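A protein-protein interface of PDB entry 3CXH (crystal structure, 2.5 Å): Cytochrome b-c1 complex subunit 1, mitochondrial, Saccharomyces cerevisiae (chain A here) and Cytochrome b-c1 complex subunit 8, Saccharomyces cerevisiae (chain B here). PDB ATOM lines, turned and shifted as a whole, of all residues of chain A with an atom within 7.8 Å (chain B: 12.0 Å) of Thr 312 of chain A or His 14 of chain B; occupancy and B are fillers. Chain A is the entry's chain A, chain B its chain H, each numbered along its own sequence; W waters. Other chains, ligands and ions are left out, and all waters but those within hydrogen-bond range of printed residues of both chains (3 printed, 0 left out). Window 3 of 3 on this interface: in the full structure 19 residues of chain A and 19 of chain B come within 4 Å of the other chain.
Printed residues of chain B within 4 Å of Thr 312 of chain A: Trp 12 (3.8 Å) and His 14 (3.5 Å).
No residue of chain B comes within 4 Å of Asn 310 of chain A.
Val 311 of chain A touches just one residue of chain B: Gly 13 (3.4 Å).
No residue of chain B comes within 4 Å of Met 313 of chain A.
No residue of chain B comes within 4 Å of Ile 314 of chain A.
No residue of chain B comes within 4 Å of Gly 415 of chain A.
Of chain A, only Val 311 and Glu 414 come within 4 Å of Gly 13 of chain B.
Of the printed residues of chain A, Gln 20 of chain B touches Arg 226 (3.3 Å).
Of the printed residues of chain A, Trp 12 of chain B touches Thr 312 (3.8 Å) and Glu 414 (3.6 Å).
Of the printed residues of chain A, Trp 11 of chain B touches Glu 414 (3.6 Å).
Of the printed residues of chain B, Arg 226 of chain A touches Gln 20 (3.3 Å).
The nearest printed residue of chain A that does not touch Met 15 of chain B is Arg 226 of chain A (6.2 Å).
The side-chain carboxylate (OE1) of Glu 414 of chain A is in hydrogen-bond range of the backbone NH (N) of Gly 13 of chain B (2.8 Å).
The side-chain carboxylate of Glu 414 of chain A is in hydrogen-bond range of the backbone NH of His 14 of chain B.
OE1 of Glu 414 of chain A is in hydrogen-bond range of N of Met 15 of chain B (2.8 Å).
The guanidinium group (NE) of Arg 226 of chain A is in hydrogen-bond range of the side-chain amide oxygen (OE1) of Gln 20 of chain B (3.3 Å).
Water W1 lies within hydrogen-bond range of O of Trp 12 of chain B (2.6 Å) and O of Thr 312 of chain A (2.8 Å).
Water W3 lies within hydrogen-bond range of the side-chain amide nitrogen of Gln 412 of chain A and the backbone carbonyl oxygen of Gly 13 of chain B.
Water W2 lies within hydrogen-bond range of the side-chain carboxylate of Glu 414 of chain A and the backbone NH of Gly 17 of chain B.
Among the printed residues, pairs that only touch across the chains: Val 311 of chain A with Gly 13 of chain B (3.4 Å), Thr 312 of chain A with Trp 12 of chain B (3.8 Å), Thr 312 of chain A with His 14 of chain B (3.5 Å), Glu 414 of chain A with Trp 11 of chain B (3.6 Å) and Glu 414 of chain A with Trp 12 of chain B (3.6 Å).
Of the 14 printed residues of chain A, 4 touch a printed residue of chain B.
Along chain A the printed residues that touch a printed residue of chain B span positions 226 to 414.
The backbone carbonyl oxygen (O) of Met 15 of chain B lies within hydrogen-bond range of the backbone NH (N) of Gly 10 of chain B, at 2.8 Å.
The guanidinium group (NH1) of Arg 226 of chain A lies within salt-bridge range of the side-chain carboxylate (OE2) of Glu 414 of chain A, at 3.3 Å.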
ATOM      1  N   ARG A 226     -13.266  18.003  23.575  1.00  0.00           N
ATOM      2  CA  ARG A 226     -12.305  17.024  24.081  1.00  0.00           C
ATOM      3  C   ARG A 226     -12.947  15.914  24.888  1.00  0.00           C
ATOM      4  O   ARG A 226     -13.747  16.171  25.775  1.00  0.00           O
ATOM      5  CB  ARG A 226     -11.197  17.668  24.923  1.00  0.00           C
ATOM      6  CG  ARG A 226      -9.878  16.879  24.831  1.00  0.00           C
ATOM      7  CD  ARG A 226      -9.188  16.602  26.166  1.00  0.00           C
ATOM      8  NE  ARG A 226      -8.116  17.553  26.442  1.00  0.00           N
ATOM      9  CZ  ARG A 226      -7.042  17.305  27.195  1.00  0.00           C
ATOM     10  NH1 ARG A 226      -6.142  18.260  27.382  1.00  0.00           N
ATOM     11  NH2 ARG A 226      -6.853  16.118  27.759  1.00  0.00           N
ATOM     12  N   LEU A 285       1.240   9.536  10.848  1.00  0.00           N
ATOM     13  CA  LEU A 285       0.542  10.638  11.487  1.00  0.00           C
ATOM     14  C   LEU A 285      -0.979  10.524  11.611  1.00  0.00           C
ATOM     15  O   LEU A 285      -1.582  11.194  12.451  1.00  0.00           O
ATOM     16  CB  LEU A 285       0.942  11.942  10.796  1.00  0.00           C
ATOM     17  CG  LEU A 285       2.167  12.680  11.353  1.00  0.00           C
ATOM     18  CD1 LEU A 285       3.159  11.753  12.025  1.00  0.00           C
ATOM     19  CD2 LEU A 285       2.816  13.487  10.253  1.00  0.00           C
ATOM     20  N   THR A 308      -6.985  10.127  13.780  1.00  0.00           N
ATOM     21  CA  THR A 308      -5.703   9.558  14.142  1.00  0.00           C
ATOM     22  C   THR A 308      -5.595   9.015  15.550  1.00  0.00           C
ATOM     23  O   THR A 308      -6.269   9.478  16.466  1.00  0.00           O
ATOM     24  CB  THR A 308      -4.569  10.560  13.939  1.00  0.00           C
ATOM     25  OG1 THR A 308      -3.355   9.997  14.448  1.00  0.00           O
ATOM     26  CG2 THR A 308      -4.867  11.858  14.662  1.00  0.00           C
ATOM     27  N   ARG A 309      -4.729   8.013  15.694  1.00  0.00           N
ATOM     28  CA  ARG A 309      -4.448   7.373  16.979  1.00  0.00           C
ATOM     29  C   ARG A 309      -3.096   7.865  17.450  1.00  0.00           C
ATOM     30  O   ARG A 309      -2.654   7.523  18.536  1.00  0.00           O
ATOM     31  CB  ARG A 309      -4.434   5.852  16.828  1.00  0.00           C
ATOM     32  CG  ARG A 309      -5.811   5.250  16.634  1.00  0.00           C
ATOM     33  CD  ARG A 309      -5.781   3.738  16.535  1.00  0.00           C
ATOM     34  NE  ARG A 309      -5.489   3.276  15.183  1.00  0.00           N
ATOM     35  CZ  ARG A 309      -4.269   3.085  14.696  1.00  0.00           C
ATOM     36  NH1 ARG A 309      -4.105   2.671  13.448  1.00  0.00           N
ATOM     37  NH2 ARG A 309      -3.210   3.315  15.451  1.00  0.00           N
ATOM     38  N   ASN A 310      -2.451   8.674  16.612  1.00  0.00           N
ATOM     39  CA  ASN A 310      -1.146   9.245  16.912  1.00  0.00           C
ATOM     40  C   ASN A 310      -1.336  10.557  17.682  1.00  0.00           C
ATOM     41  O   ASN A 310      -0.974  11.643  17.229  1.00  0.00           O
ATOM     42  CB  ASN A 310      -0.367   9.475  15.616  1.00  0.00           C
ATOM     43  CG  ASN A 310       1.129   9.484  15.836  1.00  0.00           C
ATOM     44  OD1 ASN A 310       1.903   9.225  14.916  1.00  0.00           O
ATOM     45  ND2 ASN A 310       1.546   9.766  17.066  1.00  0.00           N
ATOM     46  N   VAL A 311      -1.849  10.412  18.895  1.00  0.00           N
ATOM     47  CA  VAL A 311      -2.158  11.523  19.772  1.00  0.00           C
ATOM     48  C   VAL A 311      -1.007  12.400  20.248  1.00  0.00           C
ATOM     49  O   VAL A 311      -1.246  13.490  20.776  1.00  0.00           O
ATOM     50  CB  VAL A 311      -3.008  11.046  20.967  1.00  0.00           C
ATOM     51  CG1 VAL A 311      -4.273  10.398  20.453  1.00  0.00           C
ATOM     52  CG2 VAL A 311      -2.236  10.057  21.832  1.00  0.00           C
ATOM     53  N   THR A 312       0.235  11.958  20.044  1.00  0.00           N
ATOM     54  CA  THR A 312       1.386  12.757  20.466  1.00  0.00           C
ATOM     55  C   THR A 312       2.019  13.517  19.313  1.00  0.00           C
ATOM     56  O   THR A 312       2.961  14.287  19.521  1.00  0.00           O
ATOM     57  CB  THR A 312       2.498  11.905  21.123  1.00  0.00           C
ATOM     58  OG1 THR A 312       2.982  10.929  20.191  1.00  0.00           O
ATOM     59  CG2 THR A 312       1.990  11.230  22.373  1.00  0.00           C
ATOM     60  N   MET A 313       1.535  13.292  18.096  1.00  0.00           N
ATOM     61  CA  MET A 313       2.113  13.985  16.945  1.00  0.00           C
ATOM     62  C   MET A 313       1.097  14.706  16.067  1.00  0.00           C
ATOM     63  O   MET A 313       1.351  14.971  14.889  1.00  0.00           O
ATOM     64  CB  MET A 313       2.964  13.021  16.116  1.00  0.00           C
ATOM     65  CG  MET A 313       4.070  12.375  16.919  1.00  0.00           C
ATOM     66  SD  MET A 313       5.104  11.287  15.967  1.00  0.00           S
ATOM     67  CE  MET A 313       5.943  12.500  14.949  1.00  0.00           C
ATOM     68  N   ILE A 314      -0.041  15.051  16.658  1.00  0.00           N
ATOM     69  CA  ILE A 314      -1.094  15.766  15.950  1.00  0.00           C
ATOM     70  C   ILE A 314      -0.560  17.091  15.416  1.00  0.00           C
ATOM     71  O   ILE A 314      -0.919  17.499  14.316  1.00  0.00           O
ATOM     72  CB  ILE A 314      -2.314  16.030  16.872  1.00  0.00           C
ATOM     73  CG1 ILE A 314      -3.030  14.713  17.180  1.00  0.00           C
ATOM     74  CG2 ILE A 314      -3.266  17.029  16.246  1.00  0.00           C
ATOM     75  CD1 ILE A 314      -4.065  14.826  18.254  1.00  0.00           C
ATOM     76  N   ASP A 315       0.328  17.745  16.160  1.00  0.00           N
ATOM     77  CA  ASP A 315       0.860  19.011  15.687  1.00  0.00           C
ATOM     78  C   ASP A 315       1.602  18.851  14.357  1.00  0.00           C
ATOM     79  O   ASP A 315       1.526  19.730  13.503  1.00  0.00           O
ATOM     80  CB  ASP A 315       1.721  19.699  16.751  1.00  0.00           C
ATOM     81  CG  ASP A 315       3.015  18.968  17.021  1.00  0.00           C
ATOM     82  OD1 ASP A 315       2.953  17.820  17.518  1.00  0.00           O
ATOM     83  OD2 ASP A 315       4.095  19.544  16.736  1.00  0.00           O
ATOM     84  N   ASP A 316       2.265  17.710  14.157  1.00  0.00           N
ATOM     85  CA  ASP A 316       2.986  17.444  12.907  1.00  0.00           C
ATOM     86  C   ASP A 316       2.010  17.166  11.773  1.00  0.00           C
ATOM     87  O   ASP A 316       2.255  17.553  10.626  1.00  0.00           O
ATOM     88  CB  ASP A 316       3.937  16.255  13.054  1.00  0.00           C
ATOM     89  CG  ASP A 316       5.150  16.575  13.910  1.00  0.00           C
ATOM     90  OD1 ASP A 316       5.350  15.880  14.931  1.00  0.00           O
ATOM     91  OD2 ASP A 316       5.902  17.514  13.560  1.00  0.00           O
ATOM     92  N   GLN A 412      -9.257  12.571  21.818  1.00  0.00           N
ATOM     93  CA  GLN A 412      -7.961  12.891  22.390  1.00  0.00           C
ATOM     94  C   GLN A 412      -7.255  14.018  21.659  1.00  0.00           C
ATOM     95  O   GLN A 412      -6.212  13.813  21.030  1.00  0.00           O
ATOM     96  CB  GLN A 412      -7.092  11.640  22.441  1.00  0.00           C
ATOM     97  CG  GLN A 412      -7.550  10.654  23.496  1.00  0.00           C
ATOM     98  CD  GLN A 412      -6.603   9.489  23.640  1.00  0.00           C
ATOM     99  OE1 GLN A 412      -6.958   8.349  23.347  1.00  0.00           O
ATOM    100  NE2 GLN A 412      -5.382   9.767  24.086  1.00  0.00           N
ATOM    101  N   GLU A 414      -5.752  16.718  23.028  1.00  0.00           N
ATOM    102  CA  GLU A 414      -4.858  17.504  23.870  1.00  0.00           C
ATOM    103  C   GLU A 414      -3.673  17.995  23.058  1.00  0.00           C
ATOM    104  O   GLU A 414      -3.147  19.082  23.309  1.00  0.00           O
ATOM    105  CB  GLU A 414      -4.350  16.686  25.055  1.00  0.00           C
ATOM    106  CG  GLU A 414      -3.378  17.456  25.941  1.00  0.00           C
ATOM    107  CD  GLU A 414      -2.812  16.597  27.057  1.00  0.00           C
ATOM    108  OE1 GLU A 414      -1.725  15.998  26.858  1.00  0.00           O
ATOM    109  OE2 GLU A 414      -3.456  16.518  28.133  1.00  0.00           O
ATOM    110  N   GLY A 415      -3.271  17.187  22.079  1.00  0.00           N
ATOM    111  CA  GLY A 415      -2.149  17.528  21.229  1.00  0.00           C
ATOM    112  C   GLY A 415      -2.422  18.538  20.128  1.00  0.00           C
ATOM    113  O   GLY A 415      -1.493  18.932  19.425  1.00  0.00           O
ATOM    114  N   SER B   4      13.634   7.074  31.270  1.00  0.00           N
ATOM    115  CA  SER B   4      13.422   8.388  31.884  1.00  0.00           C
ATOM    116  C   SER B   4      12.676   8.337  33.229  1.00  0.00           C
ATOM    117  O   SER B   4      11.663   7.639  33.356  1.00  0.00           O
ATOM    118  CB  SER B   4      12.662   9.276  30.882  1.00  0.00           C
ATOM    119  OG  SER B   4      12.281  10.521  31.435  1.00  0.00           O
ATOM    120  N   GLY B   5      13.186   9.069  34.223  1.00  0.00           N
ATOM    121  CA  GLY B   5      12.542   9.119  35.531  1.00  0.00           C
ATOM    122  C   GLY B   5      11.250   9.922  35.453  1.00  0.00           C
ATOM    123  O   GLY B   5      11.283  11.118  35.175  1.00  0.00           O
ATOM    124  N   LYS B   6      10.116   9.271  35.704  1.00  0.00           N
ATOM    125  CA  LYS B   6       8.805   9.923  35.626  1.00  0.00           C
ATOM    126  C   LYS B   6       8.506  11.022  36.634  1.00  0.00           C
ATOM    127  O   LYS B   6       8.754  10.885  37.836  1.00  0.00           O
ATOM    128  CB  LYS B   6       7.676   8.888  35.625  1.00  0.00           C
ATOM    129  CG  LYS B   6       7.667   7.996  34.377  1.00  0.00           C
ATOM    130  CD  LYS B   6       7.783   8.820  33.085  1.00  0.00           C
ATOM    131  CE  LYS B   6       7.742   7.942  31.835  1.00  0.00           C
ATOM    132  NZ  LYS B   6       6.418   7.267  31.673  1.00  0.00           N
ATOM    133  N   THR B   7       7.937  12.107  36.120  1.00  0.00           N
ATOM    134  CA  THR B   7       7.590  13.267  36.924  1.00  0.00           C
ATOM    135  C   THR B   7       6.090  13.513  36.905  1.00  0.00           C
ATOM    136  O   THR B   7       5.315  12.656  36.489  1.00  0.00           O
ATOM    137  CB  THR B   7       8.299  14.536  36.408  1.00  0.00           C
ATOM    138  OG1 THR B   7       7.714  14.940  35.166  1.00  0.00           O
ATOM    139  CG2 THR B   7       9.787  14.271  36.193  1.00  0.00           C
ATOM    140  N   TYR B   8       5.692  14.708  37.318  1.00  0.00           N
ATOM    141  CA  TYR B   8       4.284  15.069  37.368  1.00  0.00           C
ATOM    142  C   TYR B   8       3.805  15.848  36.157  1.00  0.00           C
ATOM    143  O   TYR B   8       2.682  16.351  36.133  1.00  0.00           O
ATOM    144  CB  TYR B   8       3.990  15.808  38.664  1.00  0.00           C
ATOM    145  CG  TYR B   8       4.190  14.917  39.862  1.00  0.00           C
ATOM    146  CD1 TYR B   8       5.339  15.014  40.646  1.00  0.00           C
ATOM    147  CD2 TYR B   8       3.236  13.963  40.207  1.00  0.00           C
ATOM    148  CE1 TYR B   8       5.530  14.183  41.744  1.00  0.00           C
ATOM    149  CE2 TYR B   8       3.416  13.132  41.299  1.00  0.00           C
ATOM    150  CZ  TYR B   8       4.562  13.247  42.065  1.00  0.00           C
ATOM    151  OH  TYR B   8       4.733  12.430  43.159  1.00  0.00           O
ATOM    152  N   MET B   9       4.685  15.979  35.172  1.00  0.00           N
ATOM    153  CA  MET B   9       4.344  16.642  33.931  1.00  0.00           C
ATOM    154  C   MET B   9       4.805  15.783  32.756  1.00  0.00           C
ATOM    155  O   MET B   9       5.836  15.097  32.829  1.00  0.00           O
ATOM    156  CB  MET B   9       4.955  18.034  33.826  1.00  0.00           C
ATOM    157  CG  MET B   9       4.481  18.744  32.568  1.00  0.00           C
ATOM    158  SD  MET B   9       5.260  20.298  32.236  1.00  0.00           S
ATOM    159  CE  MET B   9       6.900  19.758  31.786  1.00  0.00           C
ATOM    160  N   GLY B  10       4.008  15.806  31.692  1.00  0.00           N
ATOM    161  CA  GLY B  10       4.306  15.043  30.495  1.00  0.00           C
ATOM    162  C   GLY B  10       4.570  15.982  29.336  1.00  0.00           C
ATOM    163  O   GLY B  10       5.378  16.914  29.459  1.00  0.00           O
ATOM    164  N   TRP B  11       3.886  15.743  28.219  1.00  0.00           N
ATOM    165  CA  TRP B  11       4.032  16.572  27.017  1.00  0.00           C
ATOM    166  C   TRP B  11       2.711  16.471  26.248  1.00  0.00           C
ATOM    167  O   TRP B  11       1.855  15.677  26.615  1.00  0.00           O
ATOM    168  CB  TRP B  11       5.212  16.076  26.165  1.00  0.00           C
ATOM    169  CG  TRP B  11       5.858  17.131  25.292  1.00  0.00           C
ATOM    170  CD1 TRP B  11       5.731  17.269  23.937  1.00  0.00           C
ATOM    171  CD2 TRP B  11       6.744  18.182  25.714  1.00  0.00           C
ATOM    172  NE1 TRP B  11       6.479  18.340  23.490  1.00  0.00           N
ATOM    173  CE2 TRP B  11       7.108  18.916  24.560  1.00  0.00           C
ATOM    174  CE3 TRP B  11       7.266  18.573  26.954  1.00  0.00           C
ATOM    175  CZ2 TRP B  11       7.967  20.014  24.610  1.00  0.00           C
ATOM    176  CZ3 TRP B  11       8.121  19.664  27.002  1.00  0.00           C
ATOM    177  CH2 TRP B  11       8.462  20.371  25.837  1.00  0.00           C
ATOM    178  N   TRP B  12       2.546  17.285  25.205  1.00  0.00           N
ATOM    179  CA  TRP B  12       1.319  17.305  24.402  1.00  0.00           C
ATOM    180  C   TRP B  12       0.869  15.908  24.009  1.00  0.00           C
ATOM    181  O   TRP B  12       1.610  15.189  23.350  1.00  0.00           O
ATOM    182  CB  TRP B  12       1.525  18.142  23.141  1.00  0.00           C
ATOM    183  CG  TRP B  12       1.975  19.539  23.408  1.00  0.00           C
ATOM    184  CD1 TRP B  12       3.207  20.055  23.153  1.00  0.00           C
ATOM    185  CD2 TRP B  12       1.191  20.611  23.948  1.00  0.00           C
ATOM    186  NE1 TRP B  12       3.244  21.383  23.497  1.00  0.00           N
ATOM    187  CE2 TRP B  12       2.017  21.750  23.986  1.00  0.00           C
ATOM    188  CE3 TRP B  12      -0.134  20.721  24.395  1.00  0.00           C
ATOM    189  CZ2 TRP B  12       1.562  22.996  24.450  1.00  0.00           C
ATOM    190  CZ3 TRP B  12      -0.589  21.956  24.857  1.00  0.00           C
ATOM    191  CH2 TRP B  12       0.261  23.077  24.878  1.00  0.00           C
ATOM    192  N   GLY B  13      -0.337  15.530  24.429  1.00  0.00           N
ATOM    193  CA  GLY B  13      -0.856  14.207  24.127  1.00  0.00           C
ATOM    194  C   GLY B  13      -0.882  13.286  25.339  1.00  0.00           C
ATOM    195  O   GLY B  13      -1.657  12.328  25.386  1.00  0.00           O
ATOM    196  N   HIS B  14      -0.021  13.568  26.312  1.00  0.00           N
ATOM    197  CA  HIS B  14       0.068  12.778  27.538  1.00  0.00           C
ATOM    198  C   HIS B  14       0.623  13.707  28.621  1.00  0.00           C
ATOM    199  O   HIS B  14       1.648  13.418  29.247  1.00  0.00           O
ATOM    200  CB  HIS B  14       0.983  11.548  27.328  1.00  0.00           C
ATOM    201  CG  HIS B  14       2.353  11.882  26.807  1.00  0.00           C
ATOM    202  ND1 HIS B  14       3.485  11.833  27.596  1.00  0.00           N
ATOM    203  CD2 HIS B  14       2.767  12.305  25.587  1.00  0.00           C
ATOM    204  CE1 HIS B  14       4.533  12.218  26.887  1.00  0.00           C
ATOM    205  NE2 HIS B  14       4.125  12.510  25.666  1.00  0.00           N
ATOM    206  N   MET B  15      -0.078  14.816  28.849  1.00  0.00           N
ATOM    207  CA  MET B  15       0.348  15.833  29.812  1.00  0.00           C
ATOM    208  C   MET B  15       0.437  15.385  31.274  1.00  0.00           C
ATOM    209  O   MET B  15       1.191  15.958  32.052  1.00  0.00           O
ATOM    210  CB  MET B  15      -0.538  17.082  29.684  1.00  0.00           C
ATOM    211  CG  MET B  15       0.128  18.390  30.093  1.00  0.00           C
ATOM    212  SD  MET B  15       1.481  18.927  28.998  1.00  0.00           S
ATOM    213  CE  MET B  15       0.539  19.341  27.514  1.00  0.00           C
ATOM    214  N   GLY B  16      -0.299  14.344  31.640  1.00  0.00           N
ATOM    215  CA  GLY B  16      -0.262  13.878  33.011  1.00  0.00           C
ATOM    216  C   GLY B  16      -1.459  14.331  33.828  1.00  0.00           C
ATOM    217  O   GLY B  16      -1.499  14.128  35.048  1.00  0.00           O
ATOM    218  N   GLY B  17      -2.432  14.957  33.163  1.00  0.00           N
ATOM    219  CA  GLY B  17      -3.628  15.427  33.842  1.00  0.00           C
ATOM    220  C   GLY B  17      -4.709  14.368  33.851  1.00  0.00           C
ATOM    221  O   GLY B  17      -4.508  13.280  33.309  1.00  0.00           O
ATOM    222  N   PRO B  18      -5.855  14.629  34.494  1.00  0.00           N
ATOM    223  CA  PRO B  18      -6.937  13.638  34.527  1.00  0.00           C
ATOM    224  C   PRO B  18      -7.666  13.594  33.189  1.00  0.00           C
ATOM    225  O   PRO B  18      -7.556  14.526  32.385  1.00  0.00           O
ATOM    226  CB  PRO B  18      -7.848  14.168  35.630  1.00  0.00           C
ATOM    227  CG  PRO B  18      -7.691  15.653  35.495  1.00  0.00           C
ATOM    228  CD  PRO B  18      -6.192  15.813  35.303  1.00  0.00           C
ATOM    229  N   LYS B  19      -8.371  12.493  32.934  1.00  0.00           N
ATOM    230  CA  LYS B  19      -9.134  12.353  31.697  1.00  0.00           C
ATOM    231  C   LYS B  19     -10.238  13.415  31.654  1.00  0.00           C
ATOM    232  O   LYS B  19     -10.989  13.579  32.613  1.00  0.00           O
ATOM    233  CB  LYS B  19      -9.734  10.948  31.595  1.00  0.00           C
ATOM    234  CG  LYS B  19      -8.723   9.870  31.235  1.00  0.00           C
ATOM    235  CD  LYS B  19      -9.379   8.492  31.149  1.00  0.00           C
ATOM    236  CE  LYS B  19      -8.368   7.404  30.832  1.00  0.00           C
ATOM    237  NZ  LYS B  19      -7.619   7.752  29.599  1.00  0.00           N
ATOM    238  N   GLN B  20     -10.282  14.169  30.562  1.00  0.00           N
ATOM    239  CA  GLN B  20     -11.269  15.234  30.392  1.00  0.00           C
ATOM    240  C   GLN B  20     -12.424  14.830  29.480  1.00  0.00           C
ATOM    241  O   GLN B  20     -12.208  14.392  28.345  1.00  0.00           O
ATOM    242  CB  GLN B  20     -10.609  16.492  29.816  1.00  0.00           C
ATOM    243  CG  GLN B  20      -9.486  17.093  30.653  1.00  0.00           C
ATOM    244  CD  GLN B  20      -8.895  18.335  29.996  1.00  0.00           C
ATOM    245  OE1 GLN B  20      -9.501  18.922  29.102  1.00  0.00           O
ATOM    246  NE2 GLN B  20      -7.708  18.731  30.430  1.00  0.00           N
HETATM  247  O   HOH W   1       3.778  15.447  21.905  1.00  0.00           O
HETATM  248  O   HOH W   2      -3.767  15.439  30.699  1.00  0.00           O
HETATM  249  O   HOH W   3      -4.280  12.078  24.825  1.00  0.00           O
